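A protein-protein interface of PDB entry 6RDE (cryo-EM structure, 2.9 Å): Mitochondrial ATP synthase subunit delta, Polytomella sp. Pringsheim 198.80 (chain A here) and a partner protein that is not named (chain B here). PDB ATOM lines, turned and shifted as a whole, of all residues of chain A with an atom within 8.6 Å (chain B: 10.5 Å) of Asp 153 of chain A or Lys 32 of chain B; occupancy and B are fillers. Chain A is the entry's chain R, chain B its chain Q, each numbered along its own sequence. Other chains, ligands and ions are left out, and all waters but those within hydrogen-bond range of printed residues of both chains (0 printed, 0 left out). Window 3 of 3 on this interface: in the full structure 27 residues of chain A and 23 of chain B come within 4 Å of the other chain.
Of the 16 printed residues of chain B, 5 touch a printed residue of chain A. Of the 18 printed residues of chain A, 7 touch a printed residue of chain B. Hydrophobic or aromatic side chains of chain A that line the printed part of chain B: Phe 128, Ala 150, Val 155 and Ala 159. Among the printed residues, 12 pairs touch across the chains.
The backbone carbonyl oxygen (O) of Phe 128 of chain A lies within hydrogen-bond range of the backbone NH (N) of Ala 150 of chain A, at 2.7 Å. OD1 of Asp 156 of chain A is in hydrogen-bond range of N of Ala 158 of chain A (3.0 Å). OD1 of Asp 156 of chain A sits at hydrogen-bond distance from N of Ala 159 of chain A.
Leu 27 of chain B touches Phe 128 of chain A (CD1 to CE2, 3.7 Å). CB of Ala 150 of chain A touches CD2 of Leu 27 of chain B (3.8 Å). Leu 31 of chain B touches Ala 150 of chain A (CD2 to CB, 3.7 Å). Lys 32 of chain B touches Asp 153 of chain A. Gln 154 of chain A touches Leu 31 of chain B. Gln 154 of chain A touches Phe 35 of chain B. Val 30 of chain B touches Val 155 of chain A (O to CA, 3.6 Å). NZ of Lys 32 of chain B touches O of Val 155 of chain A, 3.8 Å away. Val 30 of chain B touches Ala 159 of chain A (CG1 to C, 3.7 Å).
N of Asp 156 of chain A lies within hydrogen-bond range of O of Val 30 of chain B, 2.7 Å away. The backbone NH of Lys 32 of chain B sits at hydrogen-bond distance from the backbone carbonyl oxygen of Gln 154 of chain A (3.0 Å). OD2 of Asp 156 of chain A sits close to O of Leu 31 of chain B (3.4 Å).
Of chain A, only Asp 153 (3.4 Å), Gln 154 (3.0 Å) and Val 155 (3.8 Å) come within 4 Å of Lys 32 of chain B. No residue of chain B comes within 4 Å of Thr 151 of chain A. Val 155 of chain A touches just these residues of chain B: Val 30 and Lys 32. Printed residues of chain A within 4 Å of Leu 27 of chain B: Phe 128 and Ala 150. Of the printed residues of chain A, Phe 35 of chain B touches Gln 154 (3.4 Å). Ala 158 of chain A touches none of the printed residues of chain B. The nearest residue of chain B that does not touch Asp 153 of chain A is Phe 35 of chain B (5.7 Å). The nearest residue of chain A that does not touch Lys 32 of chain B is Asp 156 of chain A (4.2 Å).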
ATOM      1  N   LYS A 126      11.063   0.681  22.358  1.00  0.00           N
ATOM      2  CA  LYS A 126      11.124  -0.623  23.004  1.00  0.00           C
ATOM      3  C   LYS A 126       9.720  -1.045  23.402  1.00  0.00           C
ATOM      4  O   LYS A 126       9.157  -0.504  24.357  1.00  0.00           O
ATOM      5  CB  LYS A 126      12.038  -0.585  24.228  1.00  0.00           C
ATOM      6  CG  LYS A 126      13.340   0.185  24.033  1.00  0.00           C
ATOM      7  CD  LYS A 126      14.384  -0.197  25.061  1.00  0.00           C
ATOM      8  CE  LYS A 126      13.839  -0.159  26.473  1.00  0.00           C
ATOM      9  NZ  LYS A 126      14.860  -0.656  27.428  1.00  0.00           N
ATOM     10  N   PHE A 127       9.169  -2.025  22.693  1.00  0.00           N
ATOM     11  CA  PHE A 127       7.842  -2.552  22.981  1.00  0.00           C
ATOM     12  C   PHE A 127       7.971  -3.861  23.738  1.00  0.00           C
ATOM     13  O   PHE A 127       8.781  -4.710  23.366  1.00  0.00           O
ATOM     14  CB  PHE A 127       7.049  -2.794  21.697  1.00  0.00           C
ATOM     15  CG  PHE A 127       6.953  -1.602  20.800  1.00  0.00           C
ATOM     16  CD1 PHE A 127       5.911  -0.707  20.935  1.00  0.00           C
ATOM     17  CD2 PHE A 127       7.887  -1.394  19.799  1.00  0.00           C
ATOM     18  CE1 PHE A 127       5.816   0.388  20.104  1.00  0.00           C
ATOM     19  CE2 PHE A 127       7.794  -0.303  18.970  1.00  0.00           C
ATOM     20  CZ  PHE A 127       6.759   0.586  19.121  1.00  0.00           C
ATOM     21  N   PHE A 128       7.171  -4.031  24.785  1.00  0.00           N
ATOM     22  CA  PHE A 128       7.023  -5.331  25.428  1.00  0.00           C
ATOM     23  C   PHE A 128       5.912  -6.098  24.724  1.00  0.00           C
ATOM     24  O   PHE A 128       4.766  -5.646  24.686  1.00  0.00           O
ATOM     25  CB  PHE A 128       6.709  -5.190  26.913  1.00  0.00           C
ATOM     26  CG  PHE A 128       6.561  -6.504  27.621  1.00  0.00           C
ATOM     27  CD1 PHE A 128       7.675  -7.226  28.004  1.00  0.00           C
ATOM     28  CD2 PHE A 128       5.308  -7.013  27.913  1.00  0.00           C
ATOM     29  CE1 PHE A 128       7.539  -8.435  28.651  1.00  0.00           C
ATOM     30  CE2 PHE A 128       5.169  -8.214  28.556  1.00  0.00           C
ATOM     31  CZ  PHE A 128       6.281  -8.928  28.926  1.00  0.00           C
ATOM     32  N   ALA A 149       1.256  -5.846  21.669  1.00  0.00           N
ATOM     33  CA  ALA A 149       2.493  -5.101  21.865  1.00  0.00           C
ATOM     34  C   ALA A 149       2.203  -3.989  22.860  1.00  0.00           C
ATOM     35  O   ALA A 149       1.594  -2.972  22.513  1.00  0.00           O
ATOM     36  CB  ALA A 149       3.022  -4.554  20.549  1.00  0.00           C
ATOM     37  N   ALA A 150       2.624  -4.193  24.099  1.00  0.00           N
ATOM     38  CA  ALA A 150       2.504  -3.185  25.139  1.00  0.00           C
ATOM     39  C   ALA A 150       3.755  -2.322  25.124  1.00  0.00           C
ATOM     40  O   ALA A 150       4.851  -2.817  25.391  1.00  0.00           O
ATOM     41  CB  ALA A 150       2.327  -3.847  26.503  1.00  0.00           C
ATOM     42  N   THR A 151       3.601  -1.045  24.799  1.00  0.00           N
ATOM     43  CA  THR A 151       4.741  -0.142  24.851  1.00  0.00           C
ATOM     44  C   THR A 151       5.103   0.097  26.314  1.00  0.00           C
ATOM     45  O   THR A 151       4.236   0.096  27.191  1.00  0.00           O
ATOM     46  CB  THR A 151       4.415   1.161  24.123  1.00  0.00           C
ATOM     47  OG1 THR A 151       3.856   0.845  22.846  1.00  0.00           O
ATOM     48  CG2 THR A 151       5.673   1.970  23.861  1.00  0.00           C
ATOM     49  N   LEU A 152       6.398   0.254  26.586  1.00  0.00           N
ATOM     50  CA  LEU A 152       6.907   0.164  27.947  1.00  0.00           C
ATOM     51  C   LEU A 152       6.537   1.352  28.824  1.00  0.00           C
ATOM     52  O   LEU A 152       6.670   1.260  30.048  1.00  0.00           O
ATOM     53  CB  LEU A 152       8.420   0.000  27.905  1.00  0.00           C
ATOM     54  CG  LEU A 152       8.802  -1.438  27.582  1.00  0.00           C
ATOM     55  CD1 LEU A 152      10.285  -1.548  27.361  1.00  0.00           C
ATOM     56  CD2 LEU A 152       8.351  -2.352  28.708  1.00  0.00           C
ATOM     57  N   ASP A 153       6.066   2.446  28.240  1.00  0.00           N
ATOM     58  CA  ASP A 153       5.639   3.604  29.006  1.00  0.00           C
ATOM     59  C   ASP A 153       4.152   3.588  29.338  1.00  0.00           C
ATOM     60  O   ASP A 153       3.684   4.483  30.050  1.00  0.00           O
ATOM     61  CB  ASP A 153       6.016   4.883  28.248  1.00  0.00           C
ATOM     62  CG  ASP A 153       5.467   4.918  26.821  1.00  0.00           C
ATOM     63  OD1 ASP A 153       4.781   3.966  26.392  1.00  0.00           O
ATOM     64  OD2 ASP A 153       5.751   5.902  26.109  1.00  0.00           O
ATOM     65  N   GLN A 154       3.406   2.597  28.846  1.00  0.00           N
ATOM     66  CA  GLN A 154       1.970   2.515  29.069  1.00  0.00           C
ATOM     67  C   GLN A 154       1.552   1.274  29.843  1.00  0.00           C
ATOM     68  O   GLN A 154       0.350   1.023  29.994  1.00  0.00           O
ATOM     69  CB  GLN A 154       1.220   2.577  27.731  1.00  0.00           C
ATOM     70  CG  GLN A 154       1.234   1.314  26.905  1.00  0.00           C
ATOM     71  CD  GLN A 154       0.401   1.441  25.658  1.00  0.00           C
ATOM     72  OE1 GLN A 154       0.747   2.185  24.740  1.00  0.00           O
ATOM     73  NE2 GLN A 154      -0.709   0.719  25.614  1.00  0.00           N
ATOM     74  N   VAL A 155       2.494   0.505  30.342  1.00  0.00           N
ATOM     75  CA  VAL A 155       2.175  -0.647  31.170  1.00  0.00           C
ATOM     76  C   VAL A 155       1.780  -0.173  32.560  1.00  0.00           C
ATOM     77  O   VAL A 155       2.222   0.886  33.025  1.00  0.00           O
ATOM     78  CB  VAL A 155       3.365  -1.619  31.212  1.00  0.00           C
ATOM     79  CG1 VAL A 155       3.564  -2.247  29.861  1.00  0.00           C
ATOM     80  CG2 VAL A 155       4.627  -0.883  31.605  1.00  0.00           C
ATOM     81  N   ASP A 156       0.908  -0.932  33.209  1.00  0.00           N
ATOM     82  CA  ASP A 156       0.546  -0.668  34.595  1.00  0.00           C
ATOM     83  C   ASP A 156       1.587  -1.288  35.518  1.00  0.00           C
ATOM     84  O   ASP A 156       1.708  -2.516  35.555  1.00  0.00           O
ATOM     85  CB  ASP A 156      -0.828  -1.251  34.898  1.00  0.00           C
ATOM     86  CG  ASP A 156      -1.510  -0.574  36.059  1.00  0.00           C
ATOM     87  OD1 ASP A 156      -0.903  -0.482  37.141  1.00  0.00           O
ATOM     88  OD2 ASP A 156      -2.670  -0.148  35.895  1.00  0.00           O
ATOM     89  N   PRO A 157       2.339  -0.497  36.287  1.00  0.00           N
ATOM     90  CA  PRO A 157       3.314  -1.079  37.212  1.00  0.00           C
ATOM     91  C   PRO A 157       2.729  -1.469  38.557  1.00  0.00           C
ATOM     92  O   PRO A 157       3.457  -2.008  39.397  1.00  0.00           O
ATOM     93  CB  PRO A 157       4.343   0.045  37.363  1.00  0.00           C
ATOM     94  CG  PRO A 157       3.528   1.285  37.241  1.00  0.00           C
ATOM     95  CD  PRO A 157       2.380   0.976  36.307  1.00  0.00           C
ATOM     96  N   ALA A 158       1.442  -1.222  38.784  1.00  0.00           N
ATOM     97  CA  ALA A 158       0.791  -1.601  40.029  1.00  0.00           C
ATOM     98  C   ALA A 158       0.086  -2.943  39.943  1.00  0.00           C
ATOM     99  O   ALA A 158      -0.232  -3.532  40.981  1.00  0.00           O
ATOM    100  CB  ALA A 158      -0.222  -0.533  40.450  1.00  0.00           C
ATOM    101  N   ALA A 159      -0.175  -3.432  38.735  1.00  0.00           N
ATOM    102  CA  ALA A 159      -0.841  -4.710  38.544  1.00  0.00           C
ATOM    103  C   ALA A 159       0.098  -5.808  38.064  1.00  0.00           C
ATOM    104  O   ALA A 159      -0.338  -6.953  37.928  1.00  0.00           O
ATOM    105  CB  ALA A 159      -2.003  -4.556  37.561  1.00  0.00           C
ATOM    106  N   ALA A 194      11.073  -5.887  33.026  1.00  0.00           N
ATOM    107  CA  ALA A 194      11.009  -4.968  31.902  1.00  0.00           C
ATOM    108  C   ALA A 194      10.394  -3.629  32.295  1.00  0.00           C
ATOM    109  O   ALA A 194      10.110  -2.797  31.436  1.00  0.00           O
ATOM    110  CB  ALA A 194      10.220  -5.591  30.756  1.00  0.00           C
ATOM    111  N   VAL A 195      10.196  -3.394  33.587  1.00  0.00           N
ATOM    112  CA  VAL A 195       9.540  -2.166  34.016  1.00  0.00           C
ATOM    113  C   VAL A 195      10.384  -1.497  35.092  1.00  0.00           C
ATOM    114  O   VAL A 195      10.173  -0.325  35.425  1.00  0.00           O
ATOM    115  CB  VAL A 195       8.102  -2.445  34.502  1.00  0.00           C
ATOM    116  CG1 VAL A 195       8.086  -2.968  35.936  1.00  0.00           C
ATOM    117  CG2 VAL A 195       7.224  -1.211  34.338  1.00  0.00           C
ATOM    118  N   LYS A 198      14.363   0.726  33.580  1.00  0.00           N
ATOM    119  CA  LYS A 198      14.244   1.564  32.394  1.00  0.00           C
ATOM    120  C   LYS A 198      14.698   2.989  32.682  1.00  0.00           C
ATOM    121  O   LYS A 198      14.375   3.561  33.726  1.00  0.00           O
ATOM    122  CB  LYS A 198      12.802   1.557  31.886  1.00  0.00           C
ATOM    123  CG  LYS A 198      12.355   0.166  31.511  1.00  0.00           C
ATOM    124  CD  LYS A 198      13.208  -0.329  30.357  1.00  0.00           C
ATOM    125  CE  LYS A 198      12.854  -1.733  29.940  1.00  0.00           C
ATOM    126  NZ  LYS A 198      13.299  -2.711  30.957  1.00  0.00           N
ATOM    127  N   ALA A 199      15.452   3.553  31.745  1.00  0.00           N
ATOM    128  CA  ALA A 199      15.906   4.934  31.853  1.00  0.00           C
ATOM    129  C   ALA A 199      15.057   5.845  30.970  1.00  0.00           C
ATOM    130  O   ALA A 199      13.836   5.687  30.889  1.00  0.00           O
ATOM    131  CB  ALA A 199      17.378   5.043  31.477  1.00  0.00           C
ATOM    132  N   LEU B  26      -3.727 -11.569  28.931  1.00  0.00           N
ATOM    133  CA  LEU B  26      -3.173 -11.121  30.199  1.00  0.00           C
ATOM    134  C   LEU B  26      -2.304  -9.884  30.053  1.00  0.00           C
ATOM    135  O   LEU B  26      -2.082  -9.187  31.045  1.00  0.00           O
ATOM    136  CB  LEU B  26      -2.374 -12.251  30.841  1.00  0.00           C
ATOM    137  CG  LEU B  26      -3.098 -13.580  31.041  1.00  0.00           C
ATOM    138  CD1 LEU B  26      -2.108 -14.711  31.200  1.00  0.00           C
ATOM    139  CD2 LEU B  26      -4.024 -13.509  32.235  1.00  0.00           C
ATOM    140  N   LEU B  27      -1.805  -9.592  28.856  1.00  0.00           N
ATOM    141  CA  LEU B  27      -1.035  -8.369  28.676  1.00  0.00           C
ATOM    142  C   LEU B  27      -1.936  -7.149  28.543  1.00  0.00           C
ATOM    143  O   LEU B  27      -1.534  -6.044  28.921  1.00  0.00           O
ATOM    144  CB  LEU B  27      -0.117  -8.495  27.458  1.00  0.00           C
ATOM    145  CG  LEU B  27       0.879  -7.353  27.231  1.00  0.00           C
ATOM    146  CD1 LEU B  27       1.670  -7.124  28.491  1.00  0.00           C
ATOM    147  CD2 LEU B  27       1.807  -7.599  26.066  1.00  0.00           C
ATOM    148  N   ARG B  28      -3.158  -7.329  28.027  1.00  0.00           N
ATOM    149  CA  ARG B  28      -4.088  -6.209  27.906  1.00  0.00           C
ATOM    150  C   ARG B  28      -4.550  -5.711  29.266  1.00  0.00           C
ATOM    151  O   ARG B  28      -4.835  -4.519  29.421  1.00  0.00           O
ATOM    152  CB  ARG B  28      -5.302  -6.608  27.068  1.00  0.00           C
ATOM    153  CG  ARG B  28      -5.038  -6.697  25.584  1.00  0.00           C
ATOM    154  CD  ARG B  28      -6.267  -7.133  24.805  1.00  0.00           C
ATOM    155  NE  ARG B  28      -5.915  -7.855  23.584  1.00  0.00           N
ATOM    156  CZ  ARG B  28      -6.305  -9.097  23.312  1.00  0.00           C
ATOM    157  NH1 ARG B  28      -7.065  -9.756  24.173  1.00  0.00           N
ATOM    158  NH2 ARG B  28      -5.938  -9.686  22.185  1.00  0.00           N
ATOM    159  N   ASN B  29      -4.599  -6.597  30.265  1.00  0.00           N
ATOM    160  CA  ASN B  29      -5.130  -6.233  31.570  1.00  0.00           C
ATOM    161  C   ASN B  29      -4.189  -5.333  32.355  1.00  0.00           C
ATOM    162  O   ASN B  29      -4.628  -4.670  33.300  1.00  0.00           O
ATOM    163  CB  ASN B  29      -5.417  -7.490  32.391  1.00  0.00           C
ATOM    164  CG  ASN B  29      -6.287  -8.473  31.656  1.00  0.00           C
ATOM    165  OD1 ASN B  29      -7.128  -8.092  30.850  1.00  0.00           O
ATOM    166  ND2 ASN B  29      -6.109  -9.752  31.953  1.00  0.00           N
ATOM    167  N   VAL B  30      -2.910  -5.290  31.991  1.00  0.00           N
ATOM    168  CA  VAL B  30      -1.905  -4.666  32.842  1.00  0.00           C
ATOM    169  C   VAL B  30      -1.379  -3.450  32.079  1.00  0.00           C
ATOM    170  O   VAL B  30      -0.184  -3.137  32.087  1.00  0.00           O
ATOM    171  CB  VAL B  30      -0.805  -5.678  33.234  1.00  0.00           C
ATOM    172  CG1 VAL B  30      -0.015  -5.206  34.445  1.00  0.00           C
ATOM    173  CG2 VAL B  30      -1.398  -7.045  33.529  1.00  0.00           C
ATOM    174  N   LEU B  31      -2.269  -2.785  31.358  1.00  0.00           N
ATOM    175  CA  LEU B  31      -1.989  -1.475  30.792  1.00  0.00           C
ATOM    176  C   LEU B  31      -2.638  -0.393  31.650  1.00  0.00           C
ATOM    177  O   LEU B  31      -3.367  -0.673  32.605  1.00  0.00           O
ATOM    178  CB  LEU B  31      -2.499  -1.384  29.350  1.00  0.00           C
ATOM    179  CG  LEU B  31      -2.148  -2.547  28.427  1.00  0.00           C
ATOM    180  CD1 LEU B  31      -2.819  -2.387  27.079  1.00  0.00           C
ATOM    181  CD2 LEU B  31      -0.662  -2.611  28.261  1.00  0.00           C
ATOM    182  N   LYS B  32      -2.360   0.859  31.295  1.00  0.00           N
ATOM    183  CA  LYS B  32      -3.065   1.981  31.898  1.00  0.00           C
ATOM    184  C   LYS B  32      -4.516   2.010  31.428  1.00  0.00           C
ATOM    185  O   LYS B  32      -4.831   1.630  30.302  1.00  0.00           O
ATOM    186  CB  LYS B  32      -2.381   3.300  31.542  1.00  0.00           C
ATOM    187  CG  LYS B  32      -0.935   3.383  31.964  1.00  0.00           C
ATOM    188  CD  LYS B  32      -0.323   4.710  31.569  1.00  0.00           C
ATOM    189  CE  LYS B  32       1.073   4.859  32.143  1.00  0.00           C
ATOM    190  NZ  LYS B  32       1.111   4.514  33.586  1.00  0.00           N
ATOM    191  N   GLU B  33      -5.402   2.459  32.316  1.00  0.00           N
ATOM    192  CA  GLU B  33      -6.814   2.593  31.961  1.00  0.00           C
ATOM    193  C   GLU B  33      -7.121   3.604  30.848  1.00  0.00           C
ATOM    194  O   GLU B  33      -8.207   3.485  30.255  1.00  0.00           O
ATOM    195  CB  GLU B  33      -7.622   2.924  33.224  1.00  0.00           C
ATOM    196  CG  GLU B  33      -9.010   2.292  33.270  1.00  0.00           C
ATOM    197  CD  GLU B  33      -8.984   0.820  33.650  1.00  0.00           C
ATOM    198  OE1 GLU B  33      -7.933   0.333  34.107  1.00  0.00           O
ATOM    199  OE2 GLU B  33     -10.024   0.147  33.502  1.00  0.00           O
ATOM    200  N   PRO B  34      -6.289   4.614  30.546  1.00  0.00           N
ATOM    201  CA  PRO B  34      -6.381   5.226  29.207  1.00  0.00           C
ATOM    202  C   PRO B  34      -6.226   4.238  28.061  1.00  0.00           C
ATOM    203  O   PRO B  34      -6.926   4.365  27.051  1.00  0.00           O
ATOM    204  CB  PRO B  34      -5.235   6.242  29.216  1.00  0.00           C
ATOM    205  CG  PRO B  34      -5.156   6.674  30.614  1.00  0.00           C
ATOM    206  CD  PRO B  34      -5.636   5.548  31.488  1.00  0.00           C
ATOM    207  N   PHE B  35      -5.335   3.252  28.193  1.00  0.00           N
ATOM    208  CA  PHE B  35      -5.062   2.300  27.129  1.00  0.00           C
ATOM    209  C   PHE B  35      -5.746   0.958  27.313  1.00  0.00           C
ATOM    210  O   PHE B  35      -5.972   0.267  26.318  1.00  0.00           O
ATOM    211  CB  PHE B  35      -3.555   2.052  27.012  1.00  0.00           C
ATOM    212  CG  PHE B  35      -2.756   3.284  26.739  1.00  0.00           C
ATOM    213  CD1 PHE B  35      -2.654   3.782  25.454  1.00  0.00           C
ATOM    214  CD2 PHE B  35      -2.097   3.937  27.763  1.00  0.00           C
ATOM    215  CE1 PHE B  35      -1.914   4.908  25.190  1.00  0.00           C
ATOM    216  CE2 PHE B  35      -1.349   5.069  27.507  1.00  0.00           C
ATOM    217  CZ  PHE B  35      -1.257   5.554  26.215  1.00  0.00           C
ATOM    218  N   LYS B  36      -6.061   0.568  28.552  1.00  0.00           N
ATOM    219  CA  LYS B  36      -6.722  -0.713  28.792  1.00  0.00           C
ATOM    220  C   LYS B  36      -8.140  -0.709  28.243  1.00  0.00           C
ATOM    221  O   LYS B  36      -8.602  -1.718  27.697  1.00  0.00           O
ATOM    222  CB  LYS B  36      -6.722  -1.031  30.288  1.00  0.00           C
ATOM    223  CG  LYS B  36      -7.538  -2.245  30.692  1.00  0.00           C
ATOM    224  CD  LYS B  36      -7.143  -2.744  32.069  1.00  0.00           C
ATOM    225  CE  LYS B  36      -8.016  -3.904  32.502  1.00  0.00           C
ATOM    226  NZ  LYS B  36      -8.255  -4.860  31.384  1.00  0.00           N
ATOM    227  N   ALA B  37      -8.836   0.426  28.351  1.00  0.00           N
ATOM    228  CA  ALA B  37     -10.185   0.518  27.806  1.00  0.00           C
ATOM    229  C   ALA B  37     -10.175   0.521  26.284  1.00  0.00           C
ATOM    230  O   ALA B  37     -11.147   0.086  25.658  1.00  0.00           O
ATOM    231  CB  ALA B  37     -10.886   1.763  28.343  1.00  0.00           C
ATOM    232  N   LYS B  38      -9.088   1.000  25.674  1.00  0.00           N
ATOM    233  CA  LYS B  38      -8.952   0.882  24.228  1.00  0.00           C
ATOM    234  C   LYS B  38      -8.728  -0.568  23.823  1.00  0.00           C
ATOM    235  O   LYS B  38      -9.428  -1.087  22.946  1.00  0.00           O
ATOM    236  CB  LYS B  38      -7.810   1.768  23.729  1.00  0.00           C
ATOM    237  CG  LYS B  38      -7.625   1.736  22.226  1.00  0.00           C
ATOM    238  CD  LYS B  38      -8.926   2.050  21.498  1.00  0.00           C
ATOM    239  CE  LYS B  38      -8.981   1.372  20.135  1.00  0.00           C
ATOM    240  NZ  LYS B  38     -10.323   1.488  19.511  1.00  0.00           N
ATOM    241  N   ALA B  39      -7.795  -1.251  24.488  1.00  0.00           N
ATOM    242  CA  ALA B  39      -7.550  -2.666  24.238  1.00  0.00           C
ATOM    243  C   ALA B  39      -8.652  -3.566  24.779  1.00  0.00           C
ATOM    244  O   ALA B  39      -8.622  -4.772  24.520  1.00  0.00           O
ATOM    245  CB  ALA B  39      -6.209  -3.075  24.839  1.00  0.00           C
ATOM    246  N   GLN B  40      -9.608  -3.023  25.525  1.00  0.00           N
ATOM    247  CA  GLN B  40     -10.784  -3.789  25.910  1.00  0.00           C
ATOM    248  C   GLN B  40     -11.693  -4.046  24.713  1.00  0.00           C
ATOM    249  O   GLN B  40     -12.420  -5.046  24.689  1.00  0.00           O
ATOM    250  CB  GLN B  40     -11.530  -3.042  27.020  1.00  0.00           C
ATOM    251  CG  GLN B  40     -12.718  -3.767  27.617  1.00  0.00           C
ATOM    252  CD  GLN B  40     -12.369  -5.159  28.077  1.00  0.00           C
ATOM    253  OE1 GLN B  40     -12.668  -6.143  27.402  1.00  0.00           O
ATOM    254  NE2 GLN B  40     -11.743  -5.254  29.242  1.00  0.00           N
ATOM    255  N   GLN B  43     -10.908  -7.172  22.841  1.00  0.00           N
ATOM    256  CA  GLN B  43     -10.918  -8.344  23.697  1.00  0.00           C
ATOM    257  C   GLN B  43     -12.205  -9.142  23.585  1.00  0.00           C
ATOM    258  O   GLN B  43     -12.214 -10.327  23.928  1.00  0.00           O
ATOM    259  CB  GLN B  43     -10.701  -7.918  25.152  1.00  0.00           C
ATOM    260  CG  GLN B  43      -9.873  -8.876  25.978  1.00  0.00           C
ATOM    261  CD  GLN B  43      -9.328  -8.217  27.223  1.00  0.00           C
ATOM    262  OE1 GLN B  43      -8.679  -7.174  27.154  1.00  0.00           O
ATOM    263  NE2 GLN B  43      -9.611  -8.810  28.378  1.00  0.00           N
